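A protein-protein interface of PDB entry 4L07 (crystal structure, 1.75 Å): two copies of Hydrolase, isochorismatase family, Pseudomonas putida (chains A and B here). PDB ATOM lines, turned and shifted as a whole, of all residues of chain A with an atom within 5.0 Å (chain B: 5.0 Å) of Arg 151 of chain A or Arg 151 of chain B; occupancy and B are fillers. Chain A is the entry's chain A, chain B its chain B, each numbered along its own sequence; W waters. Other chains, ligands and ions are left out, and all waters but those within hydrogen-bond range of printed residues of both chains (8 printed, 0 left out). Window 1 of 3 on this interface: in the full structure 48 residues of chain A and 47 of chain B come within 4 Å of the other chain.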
ATOM      1  N   THR A 145     -25.562 -21.054  37.229  1.00  0.00           N
ATOM      2  CA  THR A 145     -25.356 -19.692  36.739  1.00  0.00           C
ATOM      3  C   THR A 145     -26.014 -19.550  35.377  1.00  0.00           C
ATOM      4  O   THR A 145     -26.216 -20.537  34.661  1.00  0.00           O
ATOM      5  CB  THR A 145     -23.860 -19.341  36.599  1.00  0.00           C
ATOM      6  OG1 THR A 145     -23.243 -20.216  35.636  1.00  0.00           O
ATOM      7  CG2 THR A 145     -23.150 -19.477  37.939  1.00  0.00           C
ATOM      8  N   THR A 146     -26.339 -18.317  35.013  1.00  0.00           N
ATOM      9  CA  THR A 146     -27.005 -18.045  33.736  1.00  0.00           C
ATOM     10  C   THR A 146     -26.306 -18.709  32.553  1.00  0.00           C
ATOM     11  O   THR A 146     -26.952 -19.383  31.741  1.00  0.00           O
ATOM     12  CB  THR A 146     -27.103 -16.538  33.482  1.00  0.00           C
ATOM     13  OG1 THR A 146     -27.498 -15.899  34.700  1.00  0.00           O
ATOM     14  CG2 THR A 146     -28.126 -16.244  32.398  1.00  0.00           C
ATOM     15  N   SER A 147     -24.989 -18.528  32.476  1.00  0.00           N
ATOM     16  CA  SER A 147     -24.212 -19.024  31.340  1.00  0.00           C
ATOM     17  C   SER A 147     -23.915 -20.518  31.400  1.00  0.00           C
ATOM     18  O   SER A 147     -23.542 -21.105  30.390  1.00  0.00           O
ATOM     19  CB  SER A 147     -22.911 -18.234  31.164  1.00  0.00           C
ATOM     20  OG  SER A 147     -22.103 -18.256  32.334  1.00  0.00           O
ATOM     21  N   GLY A 148     -24.080 -21.125  32.574  1.00  0.00           N
ATOM     22  CA  GLY A 148     -23.742 -22.535  32.767  1.00  0.00           C
ATOM     23  C   GLY A 148     -24.969 -23.414  32.876  1.00  0.00           C
ATOM     24  O   GLY A 148     -25.625 -23.719  31.871  1.00  0.00           O
ATOM     25  N   CYS A 149     -25.290 -23.806  34.109  1.00  0.00           N
ATOM     26  CA  CYS A 149     -26.402 -24.717  34.383  1.00  0.00           C
ATOM     27  C   CYS A 149     -27.771 -24.205  33.913  1.00  0.00           C
ATOM     28  O   CYS A 149     -28.588 -24.986  33.424  1.00  0.00           O
ATOM     29  CB  CYS A 149     -26.436 -25.075  35.865  1.00  0.00           C
ATOM     30  N   VAL A 150     -28.020 -22.899  34.040  1.00  0.00           N
ATOM     31  CA  VAL A 150     -29.307 -22.327  33.624  1.00  0.00           C
ATOM     32  C   VAL A 150     -29.491 -22.445  32.115  1.00  0.00           C
ATOM     33  O   VAL A 150     -30.486 -23.025  31.655  1.00  0.00           O
ATOM     34  CB  VAL A 150     -29.481 -20.860  34.074  1.00  0.00           C
ATOM     35  CG1 VAL A 150     -30.757 -20.253  33.484  1.00  0.00           C
ATOM     36  CG2 VAL A 150     -29.532 -20.785  35.590  1.00  0.00           C
ATOM     37  N   ARG A 151     -28.526 -21.931  31.349  1.00  0.00           N
ATOM     38  CA  ARG A 151     -28.612 -21.992  29.886  1.00  0.00           C
ATOM     39  C   ARG A 151     -28.727 -23.435  29.401  1.00  0.00           C
ATOM     40  O   ARG A 151     -29.516 -23.730  28.503  1.00  0.00           O
ATOM     41  CB  ARG A 151     -27.413 -21.315  29.219  1.00  0.00           C
ATOM     42  CG  ARG A 151     -27.534 -21.268  27.695  1.00  0.00           C
ATOM     43  CD  ARG A 151     -26.211 -21.628  27.049  1.00  0.00           C
ATOM     44  NE  ARG A 151     -26.296 -21.727  25.582  1.00  0.00           N
ATOM     45  CZ  ARG A 151     -26.082 -20.704  24.765  1.00  0.00           C
ATOM     46  NH1 ARG A 151     -26.163 -20.859  23.449  1.00  0.00           N
ATOM     47  NH2 ARG A 151     -25.776 -19.518  25.272  1.00  0.00           N
ATOM     48  N   ALA A 152     -27.937 -24.328  29.994  1.00  0.00           N
ATOM     49  CA  ALA A 152     -27.971 -25.749  29.618  1.00  0.00           C
ATOM     50  C   ALA A 152     -29.344 -26.370  29.873  1.00  0.00           C
ATOM     51  O   ALA A 152     -29.847 -27.177  29.066  1.00  0.00           O
ATOM     52  CB  ALA A 152     -26.879 -26.523  30.354  1.00  0.00           C
ATOM     53  N   THR A 153     -29.952 -25.992  30.996  1.00  0.00           N
ATOM     54  CA  THR A 153     -31.277 -26.485  31.387  1.00  0.00           C
ATOM     55  C   THR A 153     -32.340 -25.967  30.425  1.00  0.00           C
ATOM     56  O   THR A 153     -33.260 -26.703  30.044  1.00  0.00           O
ATOM     57  CB  THR A 153     -31.597 -26.072  32.844  1.00  0.00           C
ATOM     58  OG1 THR A 153     -30.663 -26.712  33.719  1.00  0.00           O
ATOM     59  CG2 THR A 153     -33.021 -26.463  33.259  1.00  0.00           C
ATOM     60  N   VAL A 154     -32.187 -24.707  30.023  1.00  0.00           N
ATOM     61  CA  VAL A 154     -33.117 -24.058  29.103  1.00  0.00           C
ATOM     62  C   VAL A 154     -33.097 -24.733  27.736  1.00  0.00           C
ATOM     63  O   VAL A 154     -34.153 -25.060  27.198  1.00  0.00           O
ATOM     64  CB  VAL A 154     -32.831 -22.544  28.986  1.00  0.00           C
ATOM     65  CG1 VAL A 154     -33.517 -21.930  27.765  1.00  0.00           C
ATOM     66  CG2 VAL A 154     -33.289 -21.850  30.258  1.00  0.00           C
ATOM     67  N   VAL A 155     -31.899 -24.967  27.200  1.00  0.00           N
ATOM     68  CA  VAL A 155     -31.757 -25.673  25.919  1.00  0.00           C
ATOM     69  C   VAL A 155     -32.414 -27.044  25.985  1.00  0.00           C
ATOM     70  O   VAL A 155     -33.208 -27.400  25.105  1.00  0.00           O
ATOM     71  CB  VAL A 155     -30.283 -25.782  25.477  1.00  0.00           C
ATOM     72  CG1 VAL A 155     -30.136 -26.729  24.287  1.00  0.00           C
ATOM     73  CG2 VAL A 155     -29.740 -24.402  25.134  1.00  0.00           C
ATOM     74  N   ALA A 181     -24.723 -12.657  27.376  1.00  0.00           N
ATOM     75  CA  ALA A 181     -24.582 -13.464  26.169  1.00  0.00           C
ATOM     76  C   ALA A 181     -25.576 -14.622  26.159  1.00  0.00           C
ATOM     77  O   ALA A 181     -26.204 -14.887  25.138  1.00  0.00           O
ATOM     78  CB  ALA A 181     -23.159 -13.980  26.027  1.00  0.00           C
ATOM     79  N   SER A 182     -25.730 -15.303  27.294  1.00  0.00           N
ATOM     80  CA  SER A 182     -26.671 -16.424  27.349  1.00  0.00           C
ATOM     81  C   SER A 182     -28.127 -15.980  27.272  1.00  0.00           C
ATOM     82  O   SER A 182     -28.933 -16.635  26.619  1.00  0.00           O
ATOM     83  CB  SER A 182     -26.421 -17.327  28.560  1.00  0.00           C
ATOM     84  OG  SER A 182     -25.518 -18.366  28.193  1.00  0.00           O
ATOM     85  N   ASP A 185     -28.827 -15.376  23.583  1.00  0.00           N
ATOM     86  CA  ASP A 185     -29.020 -16.636  22.860  1.00  0.00           C
ATOM     87  C   ASP A 185     -30.360 -17.288  23.186  1.00  0.00           C
ATOM     88  O   ASP A 185     -31.024 -17.825  22.295  1.00  0.00           O
ATOM     89  CB  ASP A 185     -27.890 -17.624  23.151  1.00  0.00           C
ATOM     90  CG  ASP A 185     -26.561 -17.229  22.515  1.00  0.00           C
ATOM     91  OD1 ASP A 185     -26.494 -16.293  21.673  1.00  0.00           O
ATOM     92  OD2 ASP A 185     -25.567 -17.886  22.869  1.00  0.00           O
ATOM     93  N   ILE A 186     -30.735 -17.266  24.466  1.00  0.00           N
ATOM     94  CA  ILE A 186     -32.015 -17.822  24.900  1.00  0.00           C
ATOM     95  C   ILE A 186     -33.185 -17.088  24.228  1.00  0.00           C
ATOM     96  O   ILE A 186     -34.019 -17.720  23.586  1.00  0.00           O
ATOM     97  CB  ILE A 186     -32.152 -17.837  26.441  1.00  0.00           C
ATOM     98  CG1 ILE A 186     -31.177 -18.858  27.042  1.00  0.00           C
ATOM     99  CG2 ILE A 186     -33.584 -18.163  26.852  1.00  0.00           C
ATOM    100  CD1 ILE A 186     -30.890 -18.648  28.521  1.00  0.00           C
ATOM    101  N   TYR A 190     -34.286 -20.111  22.143  1.00  0.00           N
ATOM    102  CA  TYR A 190     -34.716 -21.167  23.075  1.00  0.00           C
ATOM    103  C   TYR A 190     -35.927 -20.872  23.947  1.00  0.00           C
ATOM    104  O   TYR A 190     -36.707 -21.773  24.233  1.00  0.00           O
ATOM    105  CB  TYR A 190     -33.541 -21.627  23.949  1.00  0.00           C
ATOM    106  CG  TYR A 190     -32.313 -22.016  23.153  1.00  0.00           C
ATOM    107  CD1 TYR A 190     -32.363 -23.034  22.195  1.00  0.00           C
ATOM    108  CD2 TYR A 190     -31.107 -21.346  23.343  1.00  0.00           C
ATOM    109  CE1 TYR A 190     -31.235 -23.378  21.457  1.00  0.00           C
ATOM    110  CE2 TYR A 190     -29.980 -21.684  22.612  1.00  0.00           C
ATOM    111  CZ  TYR A 190     -30.046 -22.697  21.675  1.00  0.00           C
ATOM    112  OH  TYR A 190     -28.920 -23.024  20.947  1.00  0.00           O
ATOM    113  N   THR B 145     -24.037 -23.581  14.256  1.00  0.00           N
ATOM    114  CA  THR B 145     -23.244 -22.385  14.544  1.00  0.00           C
ATOM    115  C   THR B 145     -22.583 -22.508  15.905  1.00  0.00           C
ATOM    116  O   THR B 145     -23.065 -23.233  16.775  1.00  0.00           O
ATOM    117  CB  THR B 145     -24.097 -21.102  14.560  1.00  0.00           C
ATOM    118  OG1 THR B 145     -25.066 -21.167  15.620  1.00  0.00           O
ATOM    119  CG2 THR B 145     -24.791 -20.869  13.217  1.00  0.00           C
ATOM    120  N   THR B 146     -21.493 -21.768  16.092  1.00  0.00           N
ATOM    121  CA  THR B 146     -20.722 -21.801  17.332  1.00  0.00           C
ATOM    122  C   THR B 146     -21.605 -21.652  18.569  1.00  0.00           C
ATOM    123  O   THR B 146     -21.501 -22.445  19.512  1.00  0.00           O
ATOM    124  CB  THR B 146     -19.664 -20.687  17.342  1.00  0.00           C
ATOM    125  OG1 THR B 146     -18.997 -20.664  16.072  1.00  0.00           O
ATOM    126  CG2 THR B 146     -18.642 -20.927  18.466  1.00  0.00           C
ATOM    127  N   SER B 147     -22.482 -20.649  18.550  1.00  0.00           N
ATOM    128  CA  SER B 147     -23.304 -20.308  19.712  1.00  0.00           C
ATOM    129  C   SER B 147     -24.568 -21.146  19.829  1.00  0.00           C
ATOM    130  O   SER B 147     -25.272 -21.056  20.834  1.00  0.00           O
ATOM    131  CB  SER B 147     -23.679 -18.825  19.685  1.00  0.00           C
ATOM    132  OG  SER B 147     -24.500 -18.545  18.558  1.00  0.00           O
ATOM    133  N   GLY B 148     -24.850 -21.959  18.816  1.00  0.00           N
ATOM    134  CA  GLY B 148     -26.077 -22.748  18.783  1.00  0.00           C
ATOM    135  C   GLY B 148     -25.779 -24.231  18.898  1.00  0.00           C
ATOM    136  O   GLY B 148     -25.418 -24.727  19.977  1.00  0.00           O
ATOM    137  N   CYS B 149     -25.907 -24.928  17.772  1.00  0.00           N
ATOM    138  CA  CYS B 149     -25.688 -26.369  17.701  1.00  0.00           C
ATOM    139  C   CYS B 149     -24.291 -26.834  18.115  1.00  0.00           C
ATOM    140  O   CYS B 149     -24.162 -27.888  18.723  1.00  0.00           O
ATOM    141  CB  CYS B 149     -26.026 -26.882  16.309  1.00  0.00           C
ATOM    142  N   VAL B 150     -23.249 -26.069  17.781  1.00  0.00           N
ATOM    143  CA  VAL B 150     -21.890 -26.429  18.206  1.00  0.00           C
ATOM    144  C   VAL B 150     -21.773 -26.446  19.733  1.00  0.00           C
ATOM    145  O   VAL B 150     -21.384 -27.473  20.312  1.00  0.00           O
ATOM    146  CB  VAL B 150     -20.809 -25.514  17.589  1.00  0.00           C
ATOM    147  CG1 VAL B 150     -19.431 -25.844  18.149  1.00  0.00           C
ATOM    148  CG2 VAL B 150     -20.800 -25.658  16.079  1.00  0.00           C
ATOM    149  N   ARG B 151     -22.121 -25.326  20.370  1.00  0.00           N
ATOM    150  CA  ARG B 151     -22.054 -25.194  21.830  1.00  0.00           C
ATOM    151  C   ARG B 151     -22.881 -26.274  22.525  1.00  0.00           C
ATOM    152  O   ARG B 151     -22.405 -26.928  23.454  1.00  0.00           O
ATOM    153  CB  ARG B 151     -22.523 -23.803  22.273  1.00  0.00           C
ATOM    154  CG  ARG B 151     -22.228 -23.449  23.730  1.00  0.00           C
ATOM    155  CD  ARG B 151     -23.102 -22.285  24.171  1.00  0.00           C
ATOM    156  NE  ARG B 151     -22.732 -21.720  25.481  1.00  0.00           N
ATOM    157  CZ  ARG B 151     -23.010 -22.300  26.642  1.00  0.00           C
ATOM    158  NH1 ARG B 151     -23.636 -23.468  26.659  1.00  0.00           N
ATOM    159  NH2 ARG B 151     -22.664 -21.720  27.790  1.00  0.00           N
ATOM    160  N   ALA B 152     -24.121 -26.463  22.073  1.00  0.00           N
ATOM    161  CA  ALA B 152     -24.988 -27.487  22.657  1.00  0.00           C
ATOM    162  C   ALA B 152     -24.368 -28.886  22.544  1.00  0.00           C
ATOM    163  O   ALA B 152     -24.392 -29.669  23.502  1.00  0.00           O
ATOM    164  CB  ALA B 152     -26.370 -27.446  22.020  1.00  0.00           C
ATOM    165  N   THR B 153     -23.790 -29.186  21.383  1.00  0.00           N
ATOM    166  CA  THR B 153     -23.095 -30.460  21.172  1.00  0.00           C
ATOM    167  C   THR B 153     -21.888 -30.618  22.102  1.00  0.00           C
ATOM    168  O   THR B 153     -21.640 -31.699  22.635  1.00  0.00           O
ATOM    169  CB  THR B 153     -22.660 -30.621  19.693  1.00  0.00           C
ATOM    170  OG1 THR B 153     -23.823 -30.572  18.853  1.00  0.00           O
ATOM    171  CG2 THR B 153     -21.931 -31.946  19.467  1.00  0.00           C
ATOM    172  N   VAL B 154     -21.143 -29.535  22.306  1.00  0.00           N
ATOM    173  CA  VAL B 154     -19.974 -29.565  23.181  1.00  0.00           C
ATOM    174  C   VAL B 154     -20.379 -29.864  24.631  1.00  0.00           C
ATOM    175  O   VAL B 154     -19.764 -30.709  25.289  1.00  0.00           O
ATOM    176  CB  VAL B 154     -19.176 -28.250  23.087  1.00  0.00           C
ATOM    177  CG1 VAL B 154     -18.218 -28.103  24.260  1.00  0.00           C
ATOM    178  CG2 VAL B 154     -18.406 -28.188  21.769  1.00  0.00           C
ATOM    179  N   VAL B 155     -21.401 -29.171  25.118  1.00  0.00           N
ATOM    180  CA  VAL B 155     -21.923 -29.416  26.476  1.00  0.00           C
ATOM    181  C   VAL B 155     -22.339 -30.876  26.629  1.00  0.00           C
ATOM    182  O   VAL B 155     -21.967 -31.536  27.604  1.00  0.00           O
ATOM    183  CB  VAL B 155     -23.082 -28.467  26.827  1.00  0.00           C
ATOM    184  CG1 VAL B 155     -23.731 -28.854  28.157  1.00  0.00           C
ATOM    185  CG2 VAL B 155     -22.574 -27.034  26.899  1.00  0.00           C
ATOM    186  N   SER B 182     -19.539 -17.944  23.251  1.00  0.00           N
ATOM    187  CA  SER B 182     -19.584 -19.402  23.341  1.00  0.00           C
ATOM    188  C   SER B 182     -18.197 -20.029  23.465  1.00  0.00           C
ATOM    189  O   SER B 182     -17.995 -20.935  24.271  1.00  0.00           O
ATOM    190  CB  SER B 182     -20.369 -20.012  22.183  1.00  0.00           C
ATOM    191  OG  SER B 182     -21.751 -20.034  22.508  1.00  0.00           O
ATOM    192  N   ASP B 185     -17.072 -19.608  27.067  1.00  0.00           N
ATOM    193  CA  ASP B 185     -17.754 -20.514  27.998  1.00  0.00           C
ATOM    194  C   ASP B 185     -17.195 -21.927  27.864  1.00  0.00           C
ATOM    195  O   ASP B 185     -16.977 -22.613  28.869  1.00  0.00           O
ATOM    196  CB  ASP B 185     -19.264 -20.538  27.740  1.00  0.00           C
ATOM    197  CG  ASP B 185     -19.988 -19.307  28.275  1.00  0.00           C
ATOM    198  OD1 ASP B 185     -19.374 -18.455  28.965  1.00  0.00           O
ATOM    199  OD2 ASP B 185     -21.198 -19.201  27.997  1.00  0.00           O
ATOM    200  N   ILE B 186     -16.966 -22.350  26.619  1.00  0.00           N
ATOM    201  CA  ILE B 186     -16.404 -23.671  26.341  1.00  0.00           C
ATOM    202  C   ILE B 186     -14.996 -23.798  26.937  1.00  0.00           C
ATOM    203  O   ILE B 186     -14.724 -24.729  27.704  1.00  0.00           O
ATOM    204  CB  ILE B 186     -16.406 -23.991  24.826  1.00  0.00           C
ATOM    205  CG1 ILE B 186     -17.840 -24.227  24.332  1.00  0.00           C
ATOM    206  CG2 ILE B 186     -15.539 -25.215  24.524  1.00  0.00           C
ATOM    207  CD1 ILE B 186     -18.004 -24.067  22.828  1.00  0.00           C
ATOM    208  N   TYR B 190     -16.091 -26.522  29.481  1.00  0.00           N
ATOM    209  CA  TYR B 190     -16.532 -27.729  28.756  1.00  0.00           C
ATOM    210  C   TYR B 190     -15.493 -28.444  27.920  1.00  0.00           C
ATOM    211  O   TYR B 190     -15.570 -29.662  27.760  1.00  0.00           O
ATOM    212  CB  TYR B 190     -17.766 -27.420  27.894  1.00  0.00           C
ATOM    213  CG  TYR B 190     -18.872 -26.739  28.664  1.00  0.00           C
ATOM    214  CD1 TYR B 190     -19.463 -27.363  29.773  1.00  0.00           C
ATOM    215  CD2 TYR B 190     -19.322 -25.470  28.300  1.00  0.00           C
ATOM    216  CE1 TYR B 190     -20.476 -26.742  30.486  1.00  0.00           C
ATOM    217  CE2 TYR B 190     -20.328 -24.833  29.015  1.00  0.00           C
ATOM    218  CZ  TYR B 190     -20.896 -25.474  30.103  1.00  0.00           C
ATOM    219  OH  TYR B 190     -21.892 -24.842  30.799  1.00  0.00           O
HETATM  220  O   HOH W   1     -25.747 -24.423  24.825  1.00  0.00           O
HETATM  221  O   HOH W   2     -22.906 -17.565  22.889  1.00  0.00           O
HETATM  222  O   HOH W   3     -19.362 -18.495  31.754  1.00  0.00           O
HETATM  223  O   HOH W   4     -26.663 -16.751  19.016  1.00  0.00           O
HETATM  224  O   HOH W   5     -26.750 -23.699  22.345  1.00  0.00           O
HETATM  225  O   HOH W   6     -20.920 -21.452  30.765  1.00  0.00           O
HETATM  226  O   HOH W   7     -24.137 -24.142  29.465  1.00  0.00           O
HETATM  227  O   HOH W   8     -22.957 -17.210  27.798  1.00  0.00           O
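The backbone carbonyl oxygen (O) of Ser 147 of chain A is in hydrogen-bond range of the guanidinium group (NH2) of Arg 151 of chain B (2.8 Å). The guanidinium group (NH1) of Arg 151 of chain A lies within hydrogen-bond range of the backbone carbonyl oxygen (O) of Ser 147 of chain B (2.8 Å). The guanidinium group (NE) of Arg 151 of chain A sits close to the guanidinium group (NH1) of Arg 151 of chain B, at 3.4 Å.
The backbone NH (N) of Gly 148 of chain A lies within hydrogen-bond range of the side-chain hydroxyl (OG1) of Thr 145 of chain A (3.3 Å). The guanidinium group (NH2) of Arg 151 of chain A lies within hydrogen-bond range of the side-chain hydroxyl (OG) of Ser 182 of chain A, 3.2 Å away. The side-chain carboxylate of Asp 185 of chain A lies within salt-bridge range of the guanidinium group of Arg 151 of chain A (2.9 Å). The backbone NH of Gly 148 of chain B lies within hydrogen-bond range of the side-chain hydroxyl of Thr 145 of chain B (3.3 Å). N of Arg 151 of chain B is in hydrogen-bond range of O of Thr 146 of chain B, at 3.1 Å. NH2 of Arg 151 of chain B lies within salt-bridge range of OD2 of Asp 185 of chain B, 2.9 Å away.
Ser 147 of chain A touches Asp 185 of chain B. Tyr 190 of chain B touches Gly 148 of chain A. Asp 185 of chain A touches Ser 147 of chain B (OD2 to O, 3.8 Å). OH of Tyr 190 of chain A touches CA of Gly 148 of chain B, 3.6 Å away.
Printed residues of chain B within 4 Å of Ser 147 of chain A: Arg 151 (2.8 Å) and Asp 185 (3.7 Å). Arg 151 of chain A touches two residues of chain B. Ala 181 of chain A touches none of the printed residues of chain B. Of the printed residues of chain B, Asp 185 of chain A touches Ser 147. Printed residues of chain A within 4 Å of Ser 147 of chain B: Arg 151 and Asp 185. Of chain A, only Ser 147 (2.8 Å) and Arg 151 (3.2 Å) come within 4 Å of Arg 151 of chain B. Of the printed residues of chain A, Tyr 190 of chain B touches Gly 148 (3.6 Å). The nearest residue of chain A that does not touch Arg 151 of chain B is Ser 182 of chain A (4.4 Å).
Hydrophobic or aromatic side chains of chain B that line the printed part of chain A: Tyr 190. Of the 16 printed residues of chain A, 5 touch a printed residue of chain B. Printed residues of chain A that touch a printed residue of chain B: Ser 147, Gly 148, Arg 151, Asp 185 and Tyr 190. Hydrophobic or aromatic side chains of chain A within 4 Å of the printed part of chain B: Tyr 190. Among the printed residues, 7 pairs touch across the chains.
Ser 147 of chain A touches Arg 151 of chain B, and with the chains exchanged Arg 151 of chain A touches Ser 147 of chain B. Ser 147 of chain A touches Asp 185 of chain B, and with the chains exchanged Asp 185 of chain A touches Ser 147 of chain B. Gly 148 of chain A touches Tyr 190 of chain B, and with the chains exchanged Tyr 190 of chain A touches Gly 148 of chain B. Arg 151 of chain B touches its own counterpart, Arg 151 of chain A. Of the 7 pairs that touch across the chains among the printed residues, 7 have their exchanged pair printed and touching as well.
Water W6 lies within hydrogen-bond range of O of Ser 147 of chain A (2.7 Å) and NH2 of Arg 151 of chain B (3.5 Å). Water W2 lies within hydrogen-bond range of the side-chain carboxylate (OD2) of Asp 185 of chain A (2.7 Å) and the side-chain hydroxyl (OG) of Ser 182 of chain B (2.8 Å). Water W4 bridges the side-chain carboxylate (OD1) of Asp 185 of chain A (2.7 Å) and the side-chain hydroxyl (OG) of Ser 147 of chain B (2.8 Å). Water W7 lies within hydrogen-bond range of OH of Tyr 190 of chain B (2.7 Å), O of Gly 148 of chain A (2.9 Å), NH1 of Arg 151 of chain B (2.9 Å) and O of Ser 147 of chain A (3.2 Å). Water W3 bridges OD1 of Asp 185 of chain B (2.8 Å) and OG of Ser 147 of chain A (2.8 Å). Water W1 lies within hydrogen-bond range of NE of Arg 151 of chain A (2.9 Å) and NH1 of Arg 151 of chain B (3.0 Å).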
